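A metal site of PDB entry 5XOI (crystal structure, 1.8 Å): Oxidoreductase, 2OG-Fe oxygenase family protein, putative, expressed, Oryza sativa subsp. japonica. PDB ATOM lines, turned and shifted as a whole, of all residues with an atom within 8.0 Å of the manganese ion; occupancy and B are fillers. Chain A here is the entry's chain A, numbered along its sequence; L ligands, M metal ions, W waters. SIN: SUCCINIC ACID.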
ATOM      1  N   ARG A  48     -20.986  -1.473  -6.209  1.00  0.00           N
ATOM      2  CA  ARG A  48     -21.992  -1.942  -7.154  1.00  0.00           C
ATOM      3  C   ARG A  48     -22.844  -0.765  -7.586  1.00  0.00           C
ATOM      4  O   ARG A  48     -23.229   0.066  -6.760  1.00  0.00           O
ATOM      5  CB  ARG A  48     -22.902  -3.042  -6.555  1.00  0.00           C
ATOM      6  CG  ARG A  48     -22.194  -4.384  -6.288  1.00  0.00           C
ATOM      7  CD  ARG A  48     -21.787  -5.134  -7.585  1.00  0.00           C
ATOM      8  NE  ARG A  48     -22.948  -5.405  -8.419  1.00  0.00           N
ATOM      9  CZ  ARG A  48     -23.569  -6.578  -8.529  1.00  0.00           C
ATOM     10  NH1 ARG A  48     -23.115  -7.663  -7.899  1.00  0.00           N
ATOM     11  NH2 ARG A  48     -24.638  -6.673  -9.310  1.00  0.00           N
ATOM     12  N   ASP A  49     -23.136  -0.706  -8.886  1.00  0.00           N
ATOM     13  CA  ASP A  49     -24.024   0.327  -9.401  1.00  0.00           C
ATOM     14  C   ASP A  49     -25.375   0.236  -8.705  1.00  0.00           C
ATOM     15  O   ASP A  49     -26.049  -0.806  -8.753  1.00  0.00           O
ATOM     16  CB  ASP A  49     -24.190   0.156 -10.911  1.00  0.00           C
ATOM     17  CG  ASP A  49     -24.845   1.355 -11.582  1.00  0.00           C
ATOM     18  OD1 ASP A  49     -25.134   2.373 -10.934  1.00  0.00           O
ATOM     19  OD2 ASP A  49     -25.062   1.273 -12.811  1.00  0.00           O
ATOM     20  N   LEU A 126     -23.051 -13.866 -13.331  1.00  0.00           N
ATOM     21  CA  LEU A 126     -22.821 -13.186 -12.075  1.00  0.00           C
ATOM     22  C   LEU A 126     -23.559 -13.957 -10.985  1.00  0.00           C
ATOM     23  O   LEU A 126     -24.788 -14.090 -11.039  1.00  0.00           O
ATOM     24  CB  LEU A 126     -23.313 -11.736 -12.151  1.00  0.00           C
ATOM     25  CG  LEU A 126     -22.500 -10.678 -11.408  1.00  0.00           C
ATOM     26  CD1 LEU A 126     -23.057  -9.308 -11.707  1.00  0.00           C
ATOM     27  CD2 LEU A 126     -22.521 -10.946  -9.910  1.00  0.00           C
ATOM     28  N   ASN A 128     -24.572 -13.810  -7.239  1.00  0.00           N
ATOM     29  CA  ASN A 128     -24.760 -12.900  -6.114  1.00  0.00           C
ATOM     30  C   ASN A 128     -25.275 -13.699  -4.922  1.00  0.00           C
ATOM     31  O   ASN A 128     -26.256 -14.434  -5.054  1.00  0.00           O
ATOM     32  CB  ASN A 128     -25.781 -11.811  -6.433  1.00  0.00           C
ATOM     33  CG  ASN A 128     -25.332 -10.875  -7.535  1.00  0.00           C
ATOM     34  OD1 ASN A 128     -24.374 -10.118  -7.365  1.00  0.00           O
ATOM     35  ND2 ASN A 128     -26.040 -10.916  -8.688  1.00  0.00           N
ATOM     36  N   TYR A 130     -26.850 -12.969  -1.150  1.00  0.00           N
ATOM     37  CA  TYR A 130     -27.401 -12.009  -0.204  1.00  0.00           C
ATOM     38  C   TYR A 130     -27.672 -12.733   1.111  1.00  0.00           C
ATOM     39  O   TYR A 130     -28.345 -13.764   1.107  1.00  0.00           O
ATOM     40  CB  TYR A 130     -28.732 -11.432  -0.701  1.00  0.00           C
ATOM     41  CG  TYR A 130     -28.740 -10.765  -2.063  1.00  0.00           C
ATOM     42  CD1 TYR A 130     -28.782 -11.520  -3.223  1.00  0.00           C
ATOM     43  CD2 TYR A 130     -28.740  -9.378  -2.164  1.00  0.00           C
ATOM     44  CE1 TYR A 130     -28.813 -10.905  -4.472  1.00  0.00           C
ATOM     45  CE2 TYR A 130     -28.765  -8.750  -3.409  1.00  0.00           C
ATOM     46  CZ  TYR A 130     -28.811  -9.517  -4.551  1.00  0.00           C
ATOM     47  OH  TYR A 130     -28.837  -8.878  -5.774  1.00  0.00           O
ATOM     48  N   LEU A 136     -29.783  -4.601  -3.224  1.00  0.00           N
ATOM     49  CA  LEU A 136     -29.014  -4.152  -4.387  1.00  0.00           C
ATOM     50  C   LEU A 136     -29.825  -3.058  -5.049  1.00  0.00           C
ATOM     51  O   LEU A 136     -30.979  -3.303  -5.421  1.00  0.00           O
ATOM     52  CB  LEU A 136     -28.751  -5.302  -5.368  1.00  0.00           C
ATOM     53  CG  LEU A 136     -28.027  -4.947  -6.674  1.00  0.00           C
ATOM     54  CD1 LEU A 136     -26.621  -4.387  -6.391  1.00  0.00           C
ATOM     55  CD2 LEU A 136     -27.977  -6.116  -7.676  1.00  0.00           C
ATOM     56  N   GLY A 137     -29.243  -1.860  -5.193  1.00  0.00           N
ATOM     57  CA  GLY A 137     -29.990  -0.706  -5.667  1.00  0.00           C
ATOM     58  C   GLY A 137     -30.322  -0.750  -7.141  1.00  0.00           C
ATOM     59  O   GLY A 137     -29.799  -1.547  -7.917  1.00  0.00           O
ATOM     60  N   LEU A 138     -31.247   0.129  -7.550  1.00  0.00           N
ATOM     61  CA  LEU A 138     -31.646   0.189  -8.960  1.00  0.00           C
ATOM     62  C   LEU A 138     -30.459   0.471  -9.877  1.00  0.00           C
ATOM     63  O   LEU A 138     -29.661   1.381  -9.625  1.00  0.00           O
ATOM     64  CB  LEU A 138     -32.728   1.264  -9.163  1.00  0.00           C
ATOM     65  CG  LEU A 138     -34.068   0.984  -8.476  1.00  0.00           C
ATOM     66  CD1 LEU A 138     -35.017   2.123  -8.765  1.00  0.00           C
ATOM     67  CD2 LEU A 138     -34.652  -0.337  -8.975  1.00  0.00           C
ATOM     68  N   HIS A 139     -30.380  -0.278 -10.975  1.00  0.00           N
ATOM     69  CA  HIS A 139     -29.316  -0.109 -11.959  1.00  0.00           C
ATOM     70  C   HIS A 139     -29.760  -0.755 -13.260  1.00  0.00           C
ATOM     71  O   HIS A 139     -30.673  -1.591 -13.287  1.00  0.00           O
ATOM     72  CB  HIS A 139     -28.017  -0.775 -11.494  1.00  0.00           C
ATOM     73  CG  HIS A 139     -28.149  -2.257 -11.396  1.00  0.00           C
ATOM     74  ND1 HIS A 139     -28.741  -2.873 -10.312  1.00  0.00           N
ATOM     75  CD2 HIS A 139     -27.864  -3.246 -12.275  1.00  0.00           C
ATOM     76  CE1 HIS A 139     -28.770  -4.177 -10.518  1.00  0.00           C
ATOM     77  NE2 HIS A 139     -28.250  -4.429 -11.704  1.00  0.00           N
ATOM     78  N   GLN A 140     -29.088  -0.376 -14.336  1.00  0.00           N
ATOM     79  CA  GLN A 140     -29.202  -1.021 -15.634  1.00  0.00           C
ATOM     80  C   GLN A 140     -28.040  -1.992 -15.837  1.00  0.00           C
ATOM     81  O   GLN A 140     -26.916  -1.726 -15.408  1.00  0.00           O
ATOM     82  CB  GLN A 140     -29.190   0.021 -16.751  1.00  0.00           C
ATOM     83  CG  GLN A 140     -30.415   0.923 -16.790  1.00  0.00           C
ATOM     84  CD  GLN A 140     -30.313   1.968 -17.876  1.00  0.00           C
ATOM     85  OE1 GLN A 140     -29.357   2.767 -17.893  1.00  0.00           O
ATOM     86  NE2 GLN A 140     -31.267   1.961 -18.810  1.00  0.00           N
ATOM     87  N   ASP A 141     -28.303  -3.101 -16.531  1.00  0.00           N
ATOM     88  CA  ASP A 141     -27.238  -3.994 -16.980  1.00  0.00           C
ATOM     89  C   ASP A 141     -26.716  -3.396 -18.280  1.00  0.00           C
ATOM     90  O   ASP A 141     -27.161  -3.751 -19.375  1.00  0.00           O
ATOM     91  CB  ASP A 141     -27.734  -5.418 -17.186  1.00  0.00           C
ATOM     92  CG  ASP A 141     -27.968  -6.159 -15.861  1.00  0.00           C
ATOM     93  OD1 ASP A 141     -27.736  -5.577 -14.777  1.00  0.00           O
ATOM     94  OD2 ASP A 141     -28.379  -7.323 -15.933  1.00  0.00           O
ATOM     95  N   LYS A 142     -25.772  -2.461 -18.167  1.00  0.00           N
ATOM     96  CA  LYS A 142     -25.364  -1.671 -19.311  1.00  0.00           C
ATOM     97  C   LYS A 142     -23.890  -1.852 -19.661  1.00  0.00           C
ATOM     98  O   LYS A 142     -23.353  -1.052 -20.433  1.00  0.00           O
ATOM     99  CB  LYS A 142     -25.651  -0.191 -19.029  1.00  0.00           C
ATOM    100  CG  LYS A 142     -24.885   0.335 -17.816  1.00  0.00           C
ATOM    101  CD  LYS A 142     -25.303   1.753 -17.458  1.00  0.00           C
ATOM    102  CE  LYS A 142     -24.435   2.319 -16.344  1.00  0.00           C
ATOM    103  NZ  LYS A 142     -24.472   3.810 -16.338  1.00  0.00           N
ATOM    104  N   VAL A 155     -31.139 -10.919 -20.467  1.00  0.00           N
ATOM    105  CA  VAL A 155     -30.576 -11.312 -19.172  1.00  0.00           C
ATOM    106  C   VAL A 155     -31.440 -12.437 -18.636  1.00  0.00           C
ATOM    107  O   VAL A 155     -32.670 -12.323 -18.617  1.00  0.00           O
ATOM    108  CB  VAL A 155     -30.590 -10.118 -18.199  1.00  0.00           C
ATOM    109  CG1 VAL A 155     -30.059 -10.512 -16.819  1.00  0.00           C
ATOM    110  CG2 VAL A 155     -29.820  -8.923 -18.800  1.00  0.00           C
ATOM    111  N   SER A 157     -32.012 -14.817 -15.231  1.00  0.00           N
ATOM    112  CA  SER A 157     -31.692 -14.758 -13.801  1.00  0.00           C
ATOM    113  C   SER A 157     -32.345 -15.905 -13.048  1.00  0.00           C
ATOM    114  O   SER A 157     -33.574 -16.049 -13.061  1.00  0.00           O
ATOM    115  CB  SER A 157     -32.154 -13.410 -13.222  1.00  0.00           C
ATOM    116  OG  SER A 157     -32.223 -13.440 -11.816  1.00  0.00           O
ATOM    117  N   PHE A 166     -38.163  -7.855  -5.880  1.00  0.00           N
ATOM    118  CA  PHE A 166     -37.403  -7.410  -7.046  1.00  0.00           C
ATOM    119  C   PHE A 166     -38.103  -6.196  -7.646  1.00  0.00           C
ATOM    120  O   PHE A 166     -39.294  -6.250  -7.942  1.00  0.00           O
ATOM    121  CB  PHE A 166     -37.285  -8.552  -8.074  1.00  0.00           C
ATOM    122  CG  PHE A 166     -36.479  -8.218  -9.303  1.00  0.00           C
ATOM    123  CD1 PHE A 166     -35.084  -8.321  -9.288  1.00  0.00           C
ATOM    124  CD2 PHE A 166     -37.099  -7.869 -10.495  1.00  0.00           C
ATOM    125  CE1 PHE A 166     -34.340  -8.043 -10.417  1.00  0.00           C
ATOM    126  CE2 PHE A 166     -36.345  -7.598 -11.643  1.00  0.00           C
ATOM    127  CZ  PHE A 166     -34.967  -7.685 -11.599  1.00  0.00           C
ATOM    128  N   PHE A 190     -35.274 -10.862 -18.979  1.00  0.00           N
ATOM    129  CA  PHE A 190     -35.609  -9.589 -19.609  1.00  0.00           C
ATOM    130  C   PHE A 190     -34.698  -9.342 -20.814  1.00  0.00           C
ATOM    131  O   PHE A 190     -33.464  -9.346 -20.691  1.00  0.00           O
ATOM    132  CB  PHE A 190     -35.603  -8.397 -18.629  1.00  0.00           C
ATOM    133  CG  PHE A 190     -34.409  -8.284 -17.687  1.00  0.00           C
ATOM    134  CD1 PHE A 190     -34.338  -9.024 -16.505  1.00  0.00           C
ATOM    135  CD2 PHE A 190     -33.434  -7.307 -17.908  1.00  0.00           C
ATOM    136  CE1 PHE A 190     -33.274  -8.855 -15.609  1.00  0.00           C
ATOM    137  CE2 PHE A 190     -32.376  -7.140 -17.026  1.00  0.00           C
ATOM    138  CZ  PHE A 190     -32.286  -7.926 -15.875  1.00  0.00           C
ATOM    139  N   ARG A 195     -34.587  -4.927 -22.184  1.00  0.00           N
ATOM    140  CA  ARG A 195     -33.209  -5.293 -21.878  1.00  0.00           C
ATOM    141  C   ARG A 195     -32.535  -4.289 -20.954  1.00  0.00           C
ATOM    142  O   ARG A 195     -31.667  -4.650 -20.159  1.00  0.00           O
ATOM    143  CB  ARG A 195     -32.423  -5.462 -23.188  1.00  0.00           C
ATOM    144  CG  ARG A 195     -30.933  -5.795 -23.031  1.00  0.00           C
ATOM    145  CD  ARG A 195     -30.703  -7.000 -22.109  1.00  0.00           C
ATOM    146  NE  ARG A 195     -29.280  -7.307 -22.014  1.00  0.00           N
ATOM    147  CZ  ARG A 195     -28.457  -6.653 -21.202  1.00  0.00           C
ATOM    148  NH1 ARG A 195     -28.924  -5.682 -20.428  1.00  0.00           N
ATOM    149  NH2 ARG A 195     -27.163  -6.968 -21.151  1.00  0.00           N
ATOM    150  N   ILE A 197     -34.067  -2.290 -18.558  1.00  0.00           N
ATOM    151  CA  ILE A 197     -34.833  -1.855 -17.399  1.00  0.00           C
ATOM    152  C   ILE A 197     -33.886  -1.559 -16.240  1.00  0.00           C
ATOM    153  O   ILE A 197     -32.851  -2.213 -16.053  1.00  0.00           O
ATOM    154  CB  ILE A 197     -35.888  -2.906 -16.980  1.00  0.00           C
ATOM    155  CG1 ILE A 197     -35.237  -4.282 -16.768  1.00  0.00           C
ATOM    156  CG2 ILE A 197     -37.020  -2.931 -17.997  1.00  0.00           C
ATOM    157  CD1 ILE A 197     -36.161  -5.301 -16.068  1.00  0.00           C
ATOM    158  N   PHE A 198     -34.232  -0.541 -15.473  1.00  0.00           N
ATOM    159  CA  PHE A 198     -33.639  -0.374 -14.151  1.00  0.00           C
ATOM    160  C   PHE A 198     -34.211  -1.434 -13.223  1.00  0.00           C
ATOM    161  O   PHE A 198     -35.408  -1.727 -13.254  1.00  0.00           O
ATOM    162  CB  PHE A 198     -33.926   1.022 -13.603  1.00  0.00           C
ATOM    163  CG  PHE A 198     -33.045   2.110 -14.171  1.00  0.00           C
ATOM    164  CD1 PHE A 198     -33.381   2.713 -15.385  1.00  0.00           C
ATOM    165  CD2 PHE A 198     -31.920   2.539 -13.499  1.00  0.00           C
ATOM    166  CE1 PHE A 198     -32.580   3.716 -15.926  1.00  0.00           C
ATOM    167  CE2 PHE A 198     -31.101   3.549 -14.033  1.00  0.00           C
ATOM    168  CZ  PHE A 198     -31.433   4.132 -15.237  1.00  0.00           C
ATOM    169  N   HIS A 199     -33.376  -2.024 -12.372  1.00  0.00           N
ATOM    170  CA  HIS A 199     -33.859  -3.125 -11.546  1.00  0.00           C
ATOM    171  C   HIS A 199     -32.961  -3.300 -10.336  1.00  0.00           C
ATOM    172  O   HIS A 199     -31.845  -2.770 -10.280  1.00  0.00           O
ATOM    173  CB  HIS A 199     -33.926  -4.447 -12.351  1.00  0.00           C
ATOM    174  CG  HIS A 199     -32.618  -4.846 -12.933  1.00  0.00           C
ATOM    175  ND1 HIS A 199     -32.131  -4.304 -14.114  1.00  0.00           N
ATOM    176  CD2 HIS A 199     -31.658  -5.678 -12.485  1.00  0.00           C
ATOM    177  CE1 HIS A 199     -30.944  -4.803 -14.366  1.00  0.00           C
ATOM    178  NE2 HIS A 199     -30.620  -5.637 -13.387  1.00  0.00           N
ATOM    179  N   GLY A 200     -33.469  -4.012  -9.342  1.00  0.00           N
ATOM    180  CA  GLY A 200     -32.686  -4.232  -8.144  1.00  0.00           C
ATOM    181  C   GLY A 200     -33.455  -5.081  -7.159  1.00  0.00           C
ATOM    182  O   GLY A 200     -34.554  -5.582  -7.439  1.00  0.00           O
ATOM    183  N   ASN A 225     -28.455 -15.819  -6.257  1.00  0.00           N
ATOM    184  CA  ASN A 225     -28.896 -15.431  -7.597  1.00  0.00           C
ATOM    185  C   ASN A 225     -27.786 -15.749  -8.584  1.00  0.00           C
ATOM    186  O   ASN A 225     -26.601 -15.568  -8.284  1.00  0.00           O
ATOM    187  CB  ASN A 225     -29.244 -13.934  -7.651  1.00  0.00           C
ATOM    188  CG  ASN A 225     -29.275 -13.385  -9.067  1.00  0.00           C
ATOM    189  OD1 ASN A 225     -28.340 -12.725  -9.511  1.00  0.00           O
ATOM    190  ND2 ASN A 225     -30.357 -13.656  -9.779  1.00  0.00           N
ATOM    191  N   THR A 227     -27.040 -14.647 -12.516  1.00  0.00           N
ATOM    192  CA  THR A 227     -27.507 -13.763 -13.590  1.00  0.00           C
ATOM    193  C   THR A 227     -26.628 -13.992 -14.812  1.00  0.00           C
ATOM    194  O   THR A 227     -25.430 -13.721 -14.762  1.00  0.00           O
ATOM    195  CB  THR A 227     -27.458 -12.310 -13.114  1.00  0.00           C
ATOM    196  OG1 THR A 227     -28.507 -12.118 -12.154  1.00  0.00           O
ATOM    197  CG2 THR A 227     -27.668 -11.357 -14.273  1.00  0.00           C
HETATM  198  C1  SIN L   1     -30.862 -10.255  -8.393  1.00  0.00           C
HETATM  199  O1  SIN L   1     -31.943 -10.826  -8.644  1.00  0.00           O
HETATM  200  O2  SIN L   1     -30.240 -10.584  -7.347  1.00  0.00           O
HETATM  201  C2  SIN L   1     -30.337  -9.170  -9.313  1.00  0.00           C
HETATM  202  C3  SIN L   1     -28.825  -9.271  -9.545  1.00  0.00           C
HETATM  203  C4  SIN L   1     -28.412  -8.209 -10.536  1.00  0.00           C
HETATM  204  O3  SIN L   1     -29.311  -7.493 -11.053  1.00  0.00           O
HETATM  205  O4  SIN L   1     -27.193  -8.007 -10.827  1.00  0.00           O
HETATM  206 MN    MN M   1     -28.579  -6.299 -12.866  1.00  0.00          MN
HETATM  207  O   HOH W   1     -29.003  -8.398 -13.781  1.00  0.00           O
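The backbone carbonyl oxygen of Ile 197 lies within hydrogen-bond range of a ring nitrogen (ND1) of His 199, 2.9 Å away.
NH1 of Arg 195 lies within hydrogen-bond range of O of Asp 141, at 2.8 Å.
O of Gly 137 sits at hydrogen-bond distance from ND1 of His 139 (2.9 Å).
Along chain A the residues within 4 Å of the manganese ion span positions 139 to 199.
The manganese ion is bound by NE2 of His 199, at 2.2 Å.
OD1 of Asp 141 binds the manganese ion (2.2 Å).
A ring nitrogen (NE2) of His 139 binds the manganese ion, 2.2 Å away.
An oxygen (O3) of the ligand binds the manganese ion, 2.3 Å away.
Water W1 binds the manganese ion (2.3 Å).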
